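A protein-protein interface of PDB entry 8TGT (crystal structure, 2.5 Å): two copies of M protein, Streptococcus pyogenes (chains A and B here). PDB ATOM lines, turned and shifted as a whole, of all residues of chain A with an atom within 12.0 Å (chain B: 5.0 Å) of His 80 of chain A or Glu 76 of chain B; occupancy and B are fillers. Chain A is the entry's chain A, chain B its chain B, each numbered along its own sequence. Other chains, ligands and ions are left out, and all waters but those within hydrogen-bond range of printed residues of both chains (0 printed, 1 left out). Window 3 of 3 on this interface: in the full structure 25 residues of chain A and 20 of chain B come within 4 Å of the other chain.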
ATOM      1  N   ASP A  68      31.696  21.145   9.557  1.00  0.00           N
ATOM      2  CA  ASP A  68      32.221  20.404   8.416  1.00  0.00           C
ATOM      3  C   ASP A  68      31.103  19.864   7.536  1.00  0.00           C
ATOM      4  O   ASP A  68      31.256  19.806   6.310  1.00  0.00           O
ATOM      5  CB  ASP A  68      33.118  19.265   8.898  1.00  0.00           C
ATOM      6  CG  ASP A  68      34.504  19.739   9.285  1.00  0.00           C
ATOM      7  OD1 ASP A  68      34.774  20.952   9.151  1.00  0.00           O
ATOM      8  OD2 ASP A  68      35.321  18.904   9.727  1.00  0.00           O
ATOM      9  N   TYR A  69      29.978  19.471   8.136  1.00  0.00           N
ATOM     10  CA  TYR A  69      28.853  18.977   7.350  1.00  0.00           C
ATOM     11  C   TYR A  69      28.235  20.085   6.508  1.00  0.00           C
ATOM     12  O   TYR A  69      27.901  19.871   5.338  1.00  0.00           O
ATOM     13  CB  TYR A  69      27.804  18.357   8.273  1.00  0.00           C
ATOM     14  CG  TYR A  69      26.494  18.037   7.588  1.00  0.00           C
ATOM     15  CD1 TYR A  69      26.430  17.081   6.584  1.00  0.00           C
ATOM     16  CD2 TYR A  69      25.322  18.686   7.950  1.00  0.00           C
ATOM     17  CE1 TYR A  69      25.236  16.782   5.958  1.00  0.00           C
ATOM     18  CE2 TYR A  69      24.122  18.395   7.330  1.00  0.00           C
ATOM     19  CZ  TYR A  69      24.086  17.441   6.334  1.00  0.00           C
ATOM     20  OH  TYR A  69      22.895  17.145   5.709  1.00  0.00           O
ATOM     21  N   LEU A  70      28.077  21.279   7.085  1.00  0.00           N
ATOM     22  CA  LEU A  70      27.519  22.393   6.327  1.00  0.00           C
ATOM     23  C   LEU A  70      28.509  22.901   5.285  1.00  0.00           C
ATOM     24  O   LEU A  70      28.116  23.235   4.161  1.00  0.00           O
ATOM     25  CB  LEU A  70      27.105  23.519   7.273  1.00  0.00           C
ATOM     26  CG  LEU A  70      25.977  23.197   8.256  1.00  0.00           C
ATOM     27  CD1 LEU A  70      25.854  24.287   9.310  1.00  0.00           C
ATOM     28  CD2 LEU A  70      24.658  23.000   7.523  1.00  0.00           C
ATOM     29  N   LYS A  71      29.796  22.960   5.635  1.00  0.00           N
ATOM     30  CA  LYS A  71      30.797  23.426   4.679  1.00  0.00           C
ATOM     31  C   LYS A  71      30.935  22.460   3.508  1.00  0.00           C
ATOM     32  O   LYS A  71      31.148  22.887   2.367  1.00  0.00           O
ATOM     33  CB  LYS A  71      32.142  23.622   5.377  1.00  0.00           C
ATOM     34  N   LYS A  72      30.814  21.156   3.767  1.00  0.00           N
ATOM     35  CA  LYS A  72      30.873  20.183   2.681  1.00  0.00           C
ATOM     36  C   LYS A  72      29.599  20.215   1.846  1.00  0.00           C
ATOM     37  O   LYS A  72      29.654  20.106   0.615  1.00  0.00           O
ATOM     38  CB  LYS A  72      31.114  18.781   3.241  1.00  0.00           C
ATOM     39  N   LEU A  73      28.444  20.359   2.499  1.00  0.00           N
ATOM     40  CA  LEU A  73      27.187  20.466   1.766  1.00  0.00           C
ATOM     41  C   LEU A  73      27.143  21.740   0.931  1.00  0.00           C
ATOM     42  O   LEU A  73      26.631  21.734  -0.194  1.00  0.00           O
ATOM     43  CB  LEU A  73      26.010  20.415   2.739  1.00  0.00           C
ATOM     44  CG  LEU A  73      24.695  19.835   2.218  1.00  0.00           C
ATOM     45  CD1 LEU A  73      24.867  18.374   1.835  1.00  0.00           C
ATOM     46  CD2 LEU A  73      23.600  19.991   3.259  1.00  0.00           C
ATOM     47  N   ASP A  74      27.676  22.842   1.467  1.00  0.00           N
ATOM     48  CA  ASP A  74      27.752  24.076   0.693  1.00  0.00           C
ATOM     49  C   ASP A  74      28.750  23.947  -0.450  1.00  0.00           C
ATOM     50  O   ASP A  74      28.535  24.500  -1.536  1.00  0.00           O
ATOM     51  CB  ASP A  74      28.122  25.246   1.605  1.00  0.00           C
ATOM     52  CG  ASP A  74      28.671  26.437   0.837  1.00  0.00           C
ATOM     53  OD1 ASP A  74      27.970  26.938  -0.066  1.00  0.00           O
ATOM     54  OD2 ASP A  74      29.801  26.873   1.138  1.00  0.00           O
ATOM     55  N   HIS A  75      29.846  23.218  -0.227  1.00  0.00           N
ATOM     56  CA  HIS A  75      30.819  23.003  -1.292  1.00  0.00           C
ATOM     57  C   HIS A  75      30.229  22.164  -2.417  1.00  0.00           C
ATOM     58  O   HIS A  75      30.535  22.390  -3.594  1.00  0.00           O
ATOM     59  CB  HIS A  75      32.075  22.339  -0.729  1.00  0.00           C
ATOM     60  CG  HIS A  75      32.987  21.784  -1.778  1.00  0.00           C
ATOM     61  ND1 HIS A  75      33.699  22.585  -2.645  1.00  0.00           N
ATOM     62  CD2 HIS A  75      33.304  20.507  -2.099  1.00  0.00           C
ATOM     63  CE1 HIS A  75      34.416  21.826  -3.455  1.00  0.00           C
ATOM     64  NE2 HIS A  75      34.194  20.562  -3.145  1.00  0.00           N
ATOM     65  N   GLU A  76      29.375  21.196  -2.075  1.00  0.00           N
ATOM     66  CA  GLU A  76      28.754  20.363  -3.099  1.00  0.00           C
ATOM     67  C   GLU A  76      27.772  21.157  -3.952  1.00  0.00           C
ATOM     68  O   GLU A  76      27.641  20.891  -5.152  1.00  0.00           O
ATOM     69  CB  GLU A  76      28.052  19.172  -2.447  1.00  0.00           C
ATOM     70  CG  GLU A  76      28.989  18.047  -2.036  1.00  0.00           C
ATOM     71  CD  GLU A  76      29.900  17.605  -3.167  1.00  0.00           C
ATOM     72  OE1 GLU A  76      29.382  17.116  -4.192  1.00  0.00           O
ATOM     73  OE2 GLU A  76      31.134  17.746  -3.028  1.00  0.00           O
ATOM     74  N   HIS A  77      27.075  22.127  -3.355  1.00  0.00           N
ATOM     75  CA  HIS A  77      26.175  22.972  -4.131  1.00  0.00           C
ATOM     76  C   HIS A  77      26.944  23.799  -5.152  1.00  0.00           C
ATOM     77  O   HIS A  77      26.500  23.962  -6.294  1.00  0.00           O
ATOM     78  CB  HIS A  77      25.376  23.885  -3.201  1.00  0.00           C
ATOM     79  CG  HIS A  77      24.504  23.150  -2.231  1.00  0.00           C
ATOM     80  ND1 HIS A  77      24.264  23.607  -0.953  1.00  0.00           N
ATOM     81  CD2 HIS A  77      23.812  21.992  -2.353  1.00  0.00           C
ATOM     82  CE1 HIS A  77      23.463  22.762  -0.329  1.00  0.00           C
ATOM     83  NE2 HIS A  77      23.175  21.774  -1.157  1.00  0.00           N
ATOM     84  N   LYS A  78      28.105  24.329  -4.758  1.00  0.00           N
ATOM     85  CA  LYS A  78      28.899  25.133  -5.681  1.00  0.00           C
ATOM     86  C   LYS A  78      29.539  24.275  -6.765  1.00  0.00           C
ATOM     87  O   LYS A  78      29.726  24.745  -7.893  1.00  0.00           O
ATOM     88  CB  LYS A  78      29.970  25.909  -4.915  1.00  0.00           C
ATOM     89  CG  LYS A  78      29.420  27.016  -4.028  1.00  0.00           C
ATOM     90  CD  LYS A  78      30.500  28.025  -3.669  1.00  0.00           C
ATOM     91  CE  LYS A  78      30.759  28.045  -2.171  1.00  0.00           C
ATOM     92  NZ  LYS A  78      32.206  27.892  -1.854  1.00  0.00           N
ATOM     93  N   GLU A  79      29.879  23.023  -6.445  1.00  0.00           N
ATOM     94  CA  GLU A  79      30.452  22.137  -7.452  1.00  0.00           C
ATOM     95  C   GLU A  79      29.440  21.818  -8.546  1.00  0.00           C
ATOM     96  O   GLU A  79      29.797  21.746  -9.727  1.00  0.00           O
ATOM     97  CB  GLU A  79      30.958  20.852  -6.798  1.00  0.00           C
ATOM     98  CG  GLU A  79      32.277  21.012  -6.061  1.00  0.00           C
ATOM     99  CD  GLU A  79      33.422  21.376  -6.987  1.00  0.00           C
ATOM    100  OE1 GLU A  79      33.921  20.480  -7.700  1.00  0.00           O
ATOM    101  OE2 GLU A  79      33.823  22.559  -7.003  1.00  0.00           O
ATOM    102  N   HIS A  80      28.173  21.632  -8.173  1.00  0.00           N
ATOM    103  CA  HIS A  80      27.141  21.355  -9.165  1.00  0.00           C
ATOM    104  C   HIS A  80      26.842  22.566 -10.038  1.00  0.00           C
ATOM    105  O   HIS A  80      26.373  22.398 -11.169  1.00  0.00           O
ATOM    106  CB  HIS A  80      25.861  20.877  -8.476  1.00  0.00           C
ATOM    107  CG  HIS A  80      26.065  19.704  -7.566  1.00  0.00           C
ATOM    108  ND1 HIS A  80      27.209  18.937  -7.581  1.00  0.00           N
ATOM    109  CD2 HIS A  80      25.267  19.170  -6.611  1.00  0.00           C
ATOM    110  CE1 HIS A  80      27.109  17.982  -6.675  1.00  0.00           C
ATOM    111  NE2 HIS A  80      25.940  18.100  -6.072  1.00  0.00           N
ATOM    112  N   GLN A  81      27.103  23.778  -9.543  1.00  0.00           N
ATOM    113  CA  GLN A  81      26.923  24.967 -10.370  1.00  0.00           C
ATOM    114  C   GLN A  81      28.017  25.065 -11.425  1.00  0.00           C
ATOM    115  O   GLN A  81      27.736  25.290 -12.608  1.00  0.00           O
ATOM    116  CB  GLN A  81      26.901  26.220  -9.494  1.00  0.00           C
ATOM    117  N   LYS A  82      29.278  24.895 -11.015  1.00  0.00           N
ATOM    118  CA  LYS A  82      30.379  24.894 -11.969  1.00  0.00           C
ATOM    119  C   LYS A  82      30.329  23.692 -12.902  1.00  0.00           C
ATOM    120  O   LYS A  82      30.909  23.744 -13.992  1.00  0.00           O
ATOM    121  CB  LYS A  82      31.720  24.925 -11.231  1.00  0.00           C
ATOM    122  N   GLU A  83      29.652  22.614 -12.499  1.00  0.00           N
ATOM    123  CA  GLU A  83      29.517  21.452 -13.370  1.00  0.00           C
ATOM    124  C   GLU A  83      28.615  21.760 -14.559  1.00  0.00           C
ATOM    125  O   GLU A  83      28.962  21.464 -15.708  1.00  0.00           O
ATOM    126  CB  GLU A  83      28.977  20.262 -12.578  1.00  0.00           C
ATOM    127  CG  GLU A  83      28.560  19.081 -13.441  1.00  0.00           C
ATOM    128  CD  GLU A  83      28.942  17.747 -12.829  1.00  0.00           C
ATOM    129  OE1 GLU A  83      30.145  17.413 -12.825  1.00  0.00           O
ATOM    130  OE2 GLU A  83      28.035  17.030 -12.353  1.00  0.00           O
ATOM    131  N   GLN A  84      27.448  22.357 -14.303  1.00  0.00           N
ATOM    132  CA  GLN A  84      26.526  22.651 -15.396  1.00  0.00           C
ATOM    133  C   GLN A  84      27.059  23.769 -16.282  1.00  0.00           C
ATOM    134  O   GLN A  84      26.869  23.743 -17.503  1.00  0.00           O
ATOM    135  CB  GLN A  84      25.145  23.012 -14.842  1.00  0.00           C
ATOM    136  CG  GLN A  84      24.043  21.976 -15.097  1.00  0.00           C
ATOM    137  CD  GLN A  84      23.820  21.624 -16.569  1.00  0.00           C
ATOM    138  OE1 GLN A  84      24.426  22.200 -17.474  1.00  0.00           O
ATOM    139  NE2 GLN A  84      22.938  20.661 -16.806  1.00  0.00           N
ATOM    140  N   GLN A  85      27.728  24.759 -15.686  1.00  0.00           N
ATOM    141  CA  GLN A  85      28.305  25.839 -16.483  1.00  0.00           C
ATOM    142  C   GLN A  85      29.412  25.327 -17.395  1.00  0.00           C
ATOM    143  O   GLN A  85      29.580  25.834 -18.511  1.00  0.00           O
ATOM    144  CB  GLN A  85      28.834  26.943 -15.567  1.00  0.00           C
ATOM    145  N   GLU A  86      30.173  24.328 -16.945  1.00  0.00           N
ATOM    146  CA  GLU A  86      31.195  23.728 -17.794  1.00  0.00           C
ATOM    147  C   GLU A  86      30.589  22.819 -18.857  1.00  0.00           C
ATOM    148  O   GLU A  86      31.178  22.649 -19.930  1.00  0.00           O
ATOM    149  CB  GLU A  86      32.196  22.947 -16.941  1.00  0.00           C
ATOM    150  N   GLN A  87      29.422  22.234 -18.581  1.00  0.00           N
ATOM    151  CA  GLN A  87      28.756  21.394 -19.568  1.00  0.00           C
ATOM    152  C   GLN A  87      28.066  22.220 -20.646  1.00  0.00           C
ATOM    153  O   GLN A  87      28.002  21.791 -21.803  1.00  0.00           O
ATOM    154  CB  GLN A  87      27.742  20.477 -18.884  1.00  0.00           C
ATOM    155  CG  GLN A  87      28.363  19.346 -18.084  1.00  0.00           C
ATOM    156  CD  GLN A  87      27.367  18.665 -17.164  1.00  0.00           C
ATOM    157  OE1 GLN A  87      26.214  19.084 -17.060  1.00  0.00           O
ATOM    158  NE2 GLN A  87      27.809  17.607 -16.492  1.00  0.00           N
ATOM    159  N   GLU A  88      27.545  23.396 -20.288  1.00  0.00           N
ATOM    160  CA  GLU A  88      26.892  24.245 -21.279  1.00  0.00           C
ATOM    161  C   GLU A  88      27.907  24.848 -22.243  1.00  0.00           C
ATOM    162  O   GLU A  88      27.620  25.005 -23.435  1.00  0.00           O
ATOM    163  CB  GLU A  88      26.092  25.346 -20.581  1.00  0.00           C
ATOM    164  N   GLU A  89      29.098  25.188 -21.747  1.00  0.00           N
ATOM    165  CA  GLU A  89      30.127  25.745 -22.620  1.00  0.00           C
ATOM    166  C   GLU A  89      30.708  24.677 -23.538  1.00  0.00           C
ATOM    167  O   GLU A  89      30.959  24.936 -24.721  1.00  0.00           O
ATOM    168  CB  GLU A  89      31.229  26.395 -21.784  1.00  0.00           C
ATOM    169  N   LYS B  71      25.855   9.764   6.143  1.00  0.00           N
ATOM    170  CA  LYS B  71      24.757   9.199   5.366  1.00  0.00           C
ATOM    171  C   LYS B  71      24.086  10.264   4.507  1.00  0.00           C
ATOM    172  O   LYS B  71      23.753  10.010   3.344  1.00  0.00           O
ATOM    173  CB  LYS B  71      23.739   8.538   6.295  1.00  0.00           C
ATOM    174  CG  LYS B  71      24.146   7.161   6.792  1.00  0.00           C
ATOM    175  CD  LYS B  71      23.555   6.879   8.163  1.00  0.00           C
ATOM    176  CE  LYS B  71      22.619   5.684   8.129  1.00  0.00           C
ATOM    177  NZ  LYS B  71      23.271   4.487   7.533  1.00  0.00           N
ATOM    178  N   LYS B  72      23.883  11.462   5.060  1.00  0.00           N
ATOM    179  CA  LYS B  72      23.254  12.533   4.292  1.00  0.00           C
ATOM    180  C   LYS B  72      24.167  13.022   3.174  1.00  0.00           C
ATOM    181  O   LYS B  72      23.699  13.319   2.069  1.00  0.00           O
ATOM    182  CB  LYS B  72      22.871  13.686   5.219  1.00  0.00           C
ATOM    183  CG  LYS B  72      21.778  13.338   6.216  1.00  0.00           C
ATOM    184  CD  LYS B  72      21.887  14.180   7.477  1.00  0.00           C
ATOM    185  CE  LYS B  72      20.516  14.631   7.954  1.00  0.00           C
ATOM    186  NZ  LYS B  72      20.307  14.363   9.403  1.00  0.00           N
ATOM    187  N   LEU B  73      25.471  13.115   3.443  1.00  0.00           N
ATOM    188  CA  LEU B  73      26.411  13.513   2.400  1.00  0.00           C
ATOM    189  C   LEU B  73      26.449  12.483   1.277  1.00  0.00           C
ATOM    190  O   LEU B  73      26.527  12.843   0.096  1.00  0.00           O
ATOM    191  CB  LEU B  73      27.804  13.712   2.998  1.00  0.00           C
ATOM    192  CG  LEU B  73      28.160  15.129   3.454  1.00  0.00           C
ATOM    193  CD1 LEU B  73      29.650  15.239   3.740  1.00  0.00           C
ATOM    194  CD2 LEU B  73      27.731  16.159   2.420  1.00  0.00           C
ATOM    195  N   ASP B  74      26.395  11.196   1.628  1.00  0.00           N
ATOM    196  CA  ASP B  74      26.332  10.150   0.613  1.00  0.00           C
ATOM    197  C   ASP B  74      24.969  10.115  -0.066  1.00  0.00           C
ATOM    198  O   ASP B  74      24.871   9.736  -1.239  1.00  0.00           O
ATOM    199  CB  ASP B  74      26.656   8.794   1.241  1.00  0.00           C
ATOM    200  CG  ASP B  74      26.626   7.657   0.236  1.00  0.00           C
ATOM    201  OD1 ASP B  74      27.538   7.590  -0.614  1.00  0.00           O
ATOM    202  OD2 ASP B  74      25.697   6.823   0.304  1.00  0.00           O
ATOM    203  N   HIS B  75      23.913  10.507   0.651  1.00  0.00           N
ATOM    204  CA  HIS B  75      22.584  10.561   0.051  1.00  0.00           C
ATOM    205  C   HIS B  75      22.488  11.681  -0.976  1.00  0.00           C
ATOM    206  O   HIS B  75      21.877  11.509  -2.038  1.00  0.00           O
ATOM    207  CB  HIS B  75      21.526  10.740   1.140  1.00  0.00           C
ATOM    208  CG  HIS B  75      20.122  10.539   0.658  1.00  0.00           C
ATOM    209  ND1 HIS B  75      19.440  11.490  -0.069  1.00  0.00           N
ATOM    210  CD2 HIS B  75      19.270   9.497   0.807  1.00  0.00           C
ATOM    211  CE1 HIS B  75      18.230  11.042  -0.351  1.00  0.00           C
ATOM    212  NE2 HIS B  75      18.101   9.835   0.168  1.00  0.00           N
ATOM    213  N   GLU B  76      23.081  12.840  -0.675  1.00  0.00           N
ATOM    214  CA  GLU B  76      23.076  13.949  -1.623  1.00  0.00           C
ATOM    215  C   GLU B  76      23.811  13.571  -2.902  1.00  0.00           C
ATOM    216  O   GLU B  76      23.320  13.814  -4.010  1.00  0.00           O
ATOM    217  CB  GLU B  76      23.700  15.189  -0.972  1.00  0.00           C
ATOM    218  CG  GLU B  76      23.779  16.440  -1.855  1.00  0.00           C
ATOM    219  CD  GLU B  76      24.917  16.401  -2.866  1.00  0.00           C
ATOM    220  OE1 GLU B  76      26.065  16.708  -2.486  1.00  0.00           O
ATOM    221  OE2 GLU B  76      24.660  16.068  -4.044  1.00  0.00           O
ATOM    222  N   HIS B  77      24.998  12.973  -2.765  1.00  0.00           N
ATOM    223  CA  HIS B  77      25.778  12.597  -3.938  1.00  0.00           C
ATOM    224  C   HIS B  77      25.060  11.553  -4.781  1.00  0.00           C
ATOM    225  O   HIS B  77      25.205  11.541  -6.009  1.00  0.00           O
ATOM    226  CB  HIS B  77      27.153  12.082  -3.510  1.00  0.00           C
ATOM    227  CG  HIS B  77      28.193  12.164  -4.585  1.00  0.00           C
ATOM    228  ND1 HIS B  77      28.208  11.318  -5.672  1.00  0.00           N
ATOM    229  CD2 HIS B  77      29.252  12.993  -4.739  1.00  0.00           C
ATOM    230  CE1 HIS B  77      29.231  11.621  -6.450  1.00  0.00           C
ATOM    231  NE2 HIS B  77      29.882  12.634  -5.907  1.00  0.00           N
ATOM    232  N   LYS B  78      24.280  10.674  -4.148  1.00  0.00           N
ATOM    233  CA  LYS B  78      23.540   9.668  -4.902  1.00  0.00           C
ATOM    234  C   LYS B  78      22.452  10.312  -5.752  1.00  0.00           C
ATOM    235  O   LYS B  78      22.293   9.980  -6.932  1.00  0.00           O
ATOM    236  CB  LYS B  78      22.940   8.633  -3.951  1.00  0.00           C
ATOM    237  CG  LYS B  78      23.632   7.281  -3.985  1.00  0.00           C
ATOM    238  CD  LYS B  78      25.139   7.426  -3.851  1.00  0.00           C
ATOM    239  CE  LYS B  78      25.808   6.074  -3.679  1.00  0.00           C
ATOM    240  NZ  LYS B  78      25.144   5.260  -2.621  1.00  0.00           N
ATOM    241  N   GLU B  79      21.690  11.240  -5.166  1.00  0.00           N
ATOM    242  CA  GLU B  79      20.639  11.914  -5.919  1.00  0.00           C
ATOM    243  C   GLU B  79      21.213  12.795  -7.020  1.00  0.00           C
ATOM    244  O   GLU B  79      20.591  12.942  -8.079  1.00  0.00           O
ATOM    245  CB  GLU B  79      19.766  12.741  -4.975  1.00  0.00           C
ATOM    246  CG  GLU B  79      19.031  11.919  -3.926  1.00  0.00           C
ATOM    247  CD  GLU B  79      17.523  12.013  -4.059  1.00  0.00           C
ATOM    248  OE1 GLU B  79      17.032  12.143  -5.201  1.00  0.00           O
ATOM    249  OE2 GLU B  79      16.827  11.958  -3.022  1.00  0.00           O
ATOM    250  N   HIS B  80      22.390  13.383  -6.797  1.00  0.00           N
ATOM    251  CA  HIS B  80      23.016  14.198  -7.835  1.00  0.00           C
ATOM    252  C   HIS B  80      23.459  13.342  -9.013  1.00  0.00           C
ATOM    253  O   HIS B  80      23.264  13.723 -10.173  1.00  0.00           O
ATOM    254  CB  HIS B  80      24.204  14.966  -7.258  1.00  0.00           C
ATOM    255  CG  HIS B  80      24.998  15.707  -8.289  1.00  0.00           C
ATOM    256  ND1 HIS B  80      24.463  16.724  -9.050  1.00  0.00           N
ATOM    257  CD2 HIS B  80      26.282  15.568  -8.696  1.00  0.00           C
ATOM    258  CE1 HIS B  80      25.387  17.187  -9.874  1.00  0.00           C
ATOM    259  NE2 HIS B  80      26.500  16.502  -9.679  1.00  0.00           N
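OH of Tyr 69 of chain A touches CB of Lys 72 of chain B (3.5 Å). Leu 73 of chain B touches Lys 72 of chain A. Leu 73 of chain B touches Leu 73 of chain A. Glu 76 of chain A touches Glu 76 of chain B (CB to OE1, 3.2 Å).
Of the 10 printed residues of chain B, 4 touch a printed residue of chain A. Hydrophobic or aromatic side chains of chain B within 4 Å of the printed part of chain A: Leu 73 and His 80. Of the 22 printed residues of chain A, 6 touch a printed residue of chain B. Among the printed residues, no Asp or Glu carboxylate lies within 4 Å of a Lys or Arg side-chain nitrogen of the other chain.
Lys 72 of chain A touches Leu 73 of chain B, but with the chains exchanged Leu 73 of chain A does not touch Lys 72 of chain B (5.2 Å). Glu 76 of chain B touches its own counterpart, Glu 76 of chain A. His 80 of chain A touches Glu 76 of chain B, but with the chains exchanged Glu 76 of chain A does not touch His 80 of chain B (5.7 Å). His 80 of chain B touches its own counterpart, His 80 of chain A.
A ring nitrogen (NE2) of His 80 of chain A is in hydrogen-bond range of the side-chain carboxylate of Glu 76 of chain B (3.1 Å). A ring nitrogen (NE2) of His 80 of chain B sits at hydrogen-bond distance from a ring nitrogen (ND1) of His 80 of chain A (3.3 Å). NE2 of His 80 of chain B sits at hydrogen-bond distance from OE2 of Glu 83 of chain A (3.1 Å).
His 80 of chain A touches just these residues of chain B: Glu 76 (3.1 Å) and His 80 (3.3 Å). Of the printed residues of chain A, Glu 76 of chain B touches Glu 76 (3.2 Å) and His 80 (3.1 Å). Of chain A, only Lys 72 (3.9 Å) and Leu 73 (3.7 Å) come within 4 Å of Leu 73 of chain B. His 75 of chain B touches none of the printed residues of chain A. His 77 of chain B touches none of the printed residues of chain A. No residue of chain A comes within 4 Å of Glu 79 of chain B. Of chain A, only His 80 and Glu 83 come within 4 Å of His 80 of chain B. Printed residues of chain B within 4 Å of Glu 76 of chain A: Glu 76 (3.2 Å). Of the printed residues of chain B, Lys 72 of chain A touches Leu 73 (3.9 Å). Of the printed residues of chain B, Tyr 69 of chain A touches Lys 72 (3.5 Å). Lys 82 of chain A touches none of the printed residues of chain B. Gln 81 of chain A touches none of the printed residues of chain B. The nearest printed residue of chain B that does not touch His 80 of chain A is His 77 of chain B (5.8 Å). The nearest residue of chain A that does not touch Glu 76 of chain B is Leu 73 of chain A (4.3 Å).
ND1 of His 77 of chain A sits at hydrogen-bond distance from O of Leu 73 of chain A. A ring nitrogen (ND1) of His 80 of chain A lies close to the backbone carbonyl oxygen of Glu 76 of chain A, 3.1 Å away.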
